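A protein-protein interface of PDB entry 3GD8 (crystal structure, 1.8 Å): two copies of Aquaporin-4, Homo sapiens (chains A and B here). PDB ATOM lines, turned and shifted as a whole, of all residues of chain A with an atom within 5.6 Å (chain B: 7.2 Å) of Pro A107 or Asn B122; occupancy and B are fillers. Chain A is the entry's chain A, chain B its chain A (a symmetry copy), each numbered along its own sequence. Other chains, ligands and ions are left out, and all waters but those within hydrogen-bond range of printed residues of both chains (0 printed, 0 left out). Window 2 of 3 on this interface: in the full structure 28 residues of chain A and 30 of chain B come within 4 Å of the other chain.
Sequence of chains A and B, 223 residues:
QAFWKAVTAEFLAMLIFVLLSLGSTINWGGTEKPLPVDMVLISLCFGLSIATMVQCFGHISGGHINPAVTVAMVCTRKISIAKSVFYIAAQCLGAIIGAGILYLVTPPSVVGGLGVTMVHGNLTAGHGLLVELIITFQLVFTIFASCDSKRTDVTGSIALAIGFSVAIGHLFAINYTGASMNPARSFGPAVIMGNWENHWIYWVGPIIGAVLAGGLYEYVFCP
OG1 of Thr A106 sits at hydrogen-bond distance from OH of Tyr B176.
ND1 of His B120 is in hydrogen-bond range of N of Asn B122.
N of His B120 lies within hydrogen-bond range of O of Tyr B176 (2.9 Å).
The side-chain hydroxyl (OG1) of Thr B124 lies within hydrogen-bond range of the backbone NH (N) of His B127 (3.0 Å).
Among the printed residues, pairs that only touch across the chains: Trp A28 with His B120 (3.5 Å), Trp A28 with Tyr B176 (3.6 Å), Val A105 with Leu B123 (3.3 Å), Val A105 with His B127 (3.99 Å), Val A105 with Tyr B176 (3.8 Å), Pro A107 with Asn B122 (3.5 Å) and Pro A107 with Leu B123 (3.8 Å).
Of chain B, only Asn B122 (3.5 Å) and Leu B123 (3.8 Å) come within 4 Å of Pro A107.
Of chain A, only Pro A107 comes within 4 Å of Asn B122.
Of the printed residues of chain B, Val A105 touches Leu B123 (3.3 Å), His B127 (3.99 Å) and Tyr B176 (3.8 Å).
Printed residues of chain A within 4 Å of His B120: Trp A28 (3.5 Å).
Printed residues of chain B within 4 Å of Trp A28: His B120 and Tyr B176.
Of the printed residues of chain B, Thr A106 touches Tyr B176 (2.8 Å).
The nearest printed residue of chain B that does not touch Pro A107 is His B120 (4.7 Å).
The nearest residue of chain A that does not touch Asn B122 is Ser A109 (4.3 Å).
Of the 8 printed residues of chain A, 4 touch a printed residue of chain B.
Hydrophobic or aromatic side chains of chain B that line the printed part of chain A: His B120, Leu B123, His B127 and Tyr B176.
No position is printed for both chains.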
ATOM      1  N   TRP A  28     -19.780 -21.455  18.409  1.00  0.00           N
ATOM      2  CA  TRP A  28     -19.332 -20.098  18.676  1.00  0.00           C
ATOM      3  C   TRP A  28     -18.412 -19.981  19.898  1.00  0.00           C
ATOM      4  O   TRP A  28     -17.897 -18.897  20.174  1.00  0.00           O
ATOM      5  CB  TRP A  28     -20.541 -19.168  18.755  1.00  0.00           C
ATOM      6  CG  TRP A  28     -21.094 -18.897  17.396  1.00  0.00           C
ATOM      7  CD1 TRP A  28     -22.014 -19.641  16.715  1.00  0.00           C
ATOM      8  CD2 TRP A  28     -20.722 -17.826  16.523  1.00  0.00           C
ATOM      9  NE1 TRP A  28     -22.254 -19.084  15.482  1.00  0.00           N
ATOM     10  CE2 TRP A  28     -21.474 -17.972  15.337  1.00  0.00           C
ATOM     11  CE3 TRP A  28     -19.837 -16.754  16.630  1.00  0.00           C
ATOM     12  CZ2 TRP A  28     -21.369 -17.079  14.268  1.00  0.00           C
ATOM     13  CZ3 TRP A  28     -19.732 -15.863  15.566  1.00  0.00           C
ATOM     14  CH2 TRP A  28     -20.496 -16.037  14.401  1.00  0.00           C
ATOM     15  N   VAL A 105     -18.722 -15.963   5.393  1.00  0.00           N
ATOM     16  CA  VAL A 105     -19.370 -15.100   6.385  1.00  0.00           C
ATOM     17  C   VAL A 105     -19.079 -15.492   7.826  1.00  0.00           C
ATOM     18  O   VAL A 105     -19.454 -14.764   8.735  1.00  0.00           O
ATOM     19  CB  VAL A 105     -20.910 -14.994   6.175  1.00  0.00           C
ATOM     20  CG1 VAL A 105     -21.215 -14.449   4.778  1.00  0.00           C
ATOM     21  CG2 VAL A 105     -21.610 -16.325   6.422  1.00  0.00           C
ATOM     22  N   THR A 106     -18.421 -16.627   8.045  1.00  0.00           N
ATOM     23  CA  THR A 106     -18.185 -17.129   9.398  1.00  0.00           C
ATOM     24  C   THR A 106     -16.791 -16.704   9.884  1.00  0.00           C
ATOM     25  O   THR A 106     -15.816 -16.888   9.174  1.00  0.00           O
ATOM     26  CB  THR A 106     -18.337 -18.655   9.443  1.00  0.00           C
ATOM     27  OG1 THR A 106     -19.656 -19.007   8.980  1.00  0.00           O
ATOM     28  CG2 THR A 106     -18.142 -19.194  10.861  1.00  0.00           C
ATOM     29  N   PRO A 107     -16.694 -16.130  11.093  1.00  0.00           N
ATOM     30  CA  PRO A 107     -15.347 -15.788  11.571  1.00  0.00           C
ATOM     31  C   PRO A 107     -14.399 -16.999  11.566  1.00  0.00           C
ATOM     32  O   PRO A 107     -14.783 -18.078  12.005  1.00  0.00           O
ATOM     33  CB  PRO A 107     -15.595 -15.305  13.004  1.00  0.00           C
ATOM     34  CG  PRO A 107     -17.002 -14.829  13.006  1.00  0.00           C
ATOM     35  CD  PRO A 107     -17.732 -15.761  12.070  1.00  0.00           C
ATOM     36  N   PRO A 108     -13.160 -16.822  11.072  1.00  0.00           N
ATOM     37  CA  PRO A 108     -12.225 -17.956  11.034  1.00  0.00           C
ATOM     38  C   PRO A 108     -12.070 -18.689  12.371  1.00  0.00           C
ATOM     39  O   PRO A 108     -11.901 -19.904  12.361  1.00  0.00           O
ATOM     40  CB  PRO A 108     -10.892 -17.316  10.623  1.00  0.00           C
ATOM     41  CG  PRO A 108     -11.260 -16.021   9.968  1.00  0.00           C
ATOM     42  CD  PRO A 108     -12.592 -15.596  10.478  1.00  0.00           C
ATOM     43  N   SER A 109     -12.161 -17.970  13.493  1.00  0.00           N
ATOM     44  CA  SER A 109     -12.003 -18.563  14.830  1.00  0.00           C
ATOM     45  C   SER A 109     -13.080 -19.596  15.212  1.00  0.00           C
ATOM     46  O   SER A 109     -12.859 -20.403  16.111  1.00  0.00           O
ATOM     47  CB  SER A 109     -11.968 -17.473  15.904  1.00  0.00           C
ATOM     48  OG  SER A 109     -13.128 -16.657  15.832  1.00  0.00           O
ATOM     49  N   VAL A 110     -14.238 -19.554  14.562  1.00  0.00           N
ATOM     50  CA  VAL A 110     -15.326 -20.477  14.885  1.00  0.00           C
ATOM     51  C   VAL A 110     -15.720 -21.389  13.715  1.00  0.00           C
ATOM     52  O   VAL A 110     -16.575 -22.234  13.874  1.00  0.00           O
ATOM     53  CB  VAL A 110     -16.564 -19.719  15.438  1.00  0.00           C
ATOM     54  CG1 VAL A 110     -16.178 -18.873  16.665  1.00  0.00           C
ATOM     55  CG2 VAL A 110     -17.190 -18.826  14.363  1.00  0.00           C
ATOM     56  N   VAL A 111     -15.083 -21.236  12.554  1.00  0.00           N
ATOM     57  CA  VAL A 111     -15.353 -22.116  11.408  1.00  0.00           C
ATOM     58  C   VAL A 111     -15.271 -23.591  11.788  1.00  0.00           C
ATOM     59  O   VAL A 111     -16.119 -24.396  11.376  1.00  0.00           O
ATOM     60  CB  VAL A 111     -14.384 -21.843  10.233  1.00  0.00           C
ATOM     61  CG1 VAL A 111     -14.374 -23.024   9.228  1.00  0.00           C
ATOM     62  CG2 VAL A 111     -14.782 -20.576   9.540  1.00  0.00           C
ATOM     63  N   VAL B 119     -25.151  -7.120  14.657  1.00  0.00           N
ATOM     64  CA  VAL B 119     -24.152  -7.890  13.934  1.00  0.00           C
ATOM     65  C   VAL B 119     -23.047  -8.332  14.901  1.00  0.00           C
ATOM     66  O   VAL B 119     -22.553  -7.534  15.706  1.00  0.00           O
ATOM     67  CB  VAL B 119     -23.560  -7.065  12.775  1.00  0.00           C
ATOM     68  CG1 VAL B 119     -22.507  -7.892  11.991  1.00  0.00           C
ATOM     69  CG2 VAL B 119     -24.676  -6.579  11.840  1.00  0.00           C
ATOM     70  N   HIS B 120     -22.673  -9.603  14.828  1.00  0.00           N
ATOM     71  CA  HIS B 120     -21.557 -10.111  15.621  1.00  0.00           C
ATOM     72  C   HIS B 120     -20.317  -9.237  15.411  1.00  0.00           C
ATOM     73  O   HIS B 120     -20.062  -8.763  14.298  1.00  0.00           O
ATOM     74  CB  HIS B 120     -21.226 -11.555  15.260  1.00  0.00           C
ATOM     75  CG  HIS B 120     -20.401 -12.249  16.296  1.00  0.00           C
ATOM     76  ND1 HIS B 120     -19.026 -12.154  16.338  1.00  0.00           N
ATOM     77  CD2 HIS B 120     -20.757 -13.016  17.355  1.00  0.00           C
ATOM     78  CE1 HIS B 120     -18.570 -12.839  17.370  1.00  0.00           C
ATOM     79  NE2 HIS B 120     -19.602 -13.372  18.003  1.00  0.00           N
ATOM     80  N   GLY B 121     -19.553  -9.029  16.481  1.00  0.00           N
ATOM     81  CA  GLY B 121     -18.339  -8.225  16.405  1.00  0.00           C
ATOM     82  C   GLY B 121     -17.330  -8.726  15.380  1.00  0.00           C
ATOM     83  O   GLY B 121     -16.579  -7.928  14.810  1.00  0.00           O
ATOM     84  N   ASN B 122     -17.283 -10.043  15.163  1.00  0.00           N
ATOM     85  CA  ASN B 122     -16.336 -10.633  14.209  1.00  0.00           C
ATOM     86  C   ASN B 122     -16.920 -10.790  12.791  1.00  0.00           C
ATOM     87  O   ASN B 122     -16.292 -11.404  11.924  1.00  0.00           O
ATOM     88  CB  ASN B 122     -15.798 -11.977  14.722  1.00  0.00           C
ATOM     89  CG  ASN B 122     -14.764 -11.822  15.842  1.00  0.00           C
ATOM     90  OD1 ASN B 122     -13.996 -10.868  15.868  1.00  0.00           O
ATOM     91  ND2 ASN B 122     -14.736 -12.786  16.759  1.00  0.00           N
ATOM     92  N   LEU B 123     -18.111 -10.235  12.566  1.00  0.00           N
ATOM     93  CA  LEU B 123     -18.674 -10.071  11.213  1.00  0.00           C
ATOM     94  C   LEU B 123     -18.581  -8.640  10.746  1.00  0.00           C
ATOM     95  O   LEU B 123     -18.619  -7.696  11.541  1.00  0.00           O
ATOM     96  CB  LEU B 123     -20.156 -10.498  11.168  1.00  0.00           C
ATOM     97  CG  LEU B 123     -20.521 -11.821  10.501  1.00  0.00           C
ATOM     98  CD1 LEU B 123     -20.210 -12.990  11.405  1.00  0.00           C
ATOM     99  CD2 LEU B 123     -22.005 -11.835  10.117  1.00  0.00           C
ATOM    100  N   THR B 124     -18.443  -8.447   9.442  1.00  0.00           N
ATOM    101  CA  THR B 124     -18.594  -7.110   8.874  1.00  0.00           C
ATOM    102  C   THR B 124     -20.073  -6.815   8.643  1.00  0.00           C
ATOM    103  O   THR B 124     -20.895  -7.736   8.543  1.00  0.00           O
ATOM    104  CB  THR B 124     -17.870  -6.968   7.516  1.00  0.00           C
ATOM    105  OG1 THR B 124     -18.526  -7.797   6.546  1.00  0.00           O
ATOM    106  CG2 THR B 124     -16.402  -7.358   7.635  1.00  0.00           C
ATOM    107  N   HIS B 127     -21.178  -8.638   5.479  1.00  0.00           N
ATOM    108  CA  HIS B 127     -21.525 -10.052   5.670  1.00  0.00           C
ATOM    109  C   HIS B 127     -22.835 -10.204   6.427  1.00  0.00           C
ATOM    110  O   HIS B 127     -23.644 -11.086   6.100  1.00  0.00           O
ATOM    111  CB  HIS B 127     -20.372 -10.819   6.324  1.00  0.00           C
ATOM    112  CG  HIS B 127     -19.220 -11.046   5.393  1.00  0.00           C
ATOM    113  ND1 HIS B 127     -17.936 -11.265   5.832  1.00  0.00           N
ATOM    114  CD2 HIS B 127     -19.158 -11.054   4.038  1.00  0.00           C
ATOM    115  CE1 HIS B 127     -17.133 -11.412   4.794  1.00  0.00           C
ATOM    116  NE2 HIS B 127     -17.852 -11.299   3.691  1.00  0.00           N
ATOM    117  N   TYR B 176     -25.006 -14.589  14.247  1.00  0.00           N
ATOM    118  CA  TYR B 176     -24.400 -13.800  13.172  1.00  0.00           C
ATOM    119  C   TYR B 176     -24.940 -12.369  13.167  1.00  0.00           C
ATOM    120  O   TYR B 176     -24.180 -11.403  13.151  1.00  0.00           O
ATOM    121  CB  TYR B 176     -24.686 -14.450  11.804  1.00  0.00           C
ATOM    122  CG  TYR B 176     -23.918 -15.723  11.514  1.00  0.00           C
ATOM    123  CD1 TYR B 176     -22.765 -15.699  10.735  1.00  0.00           C
ATOM    124  CD2 TYR B 176     -24.363 -16.956  11.992  1.00  0.00           C
ATOM    125  CE1 TYR B 176     -22.063 -16.853  10.471  1.00  0.00           C
ATOM    126  CE2 TYR B 176     -23.676 -18.118  11.732  1.00  0.00           C
ATOM    127  CZ  TYR B 176     -22.523 -18.061  10.957  1.00  0.00           C
ATOM    128  OH  TYR B 176     -21.812 -19.201  10.692  1.00  0.00           O
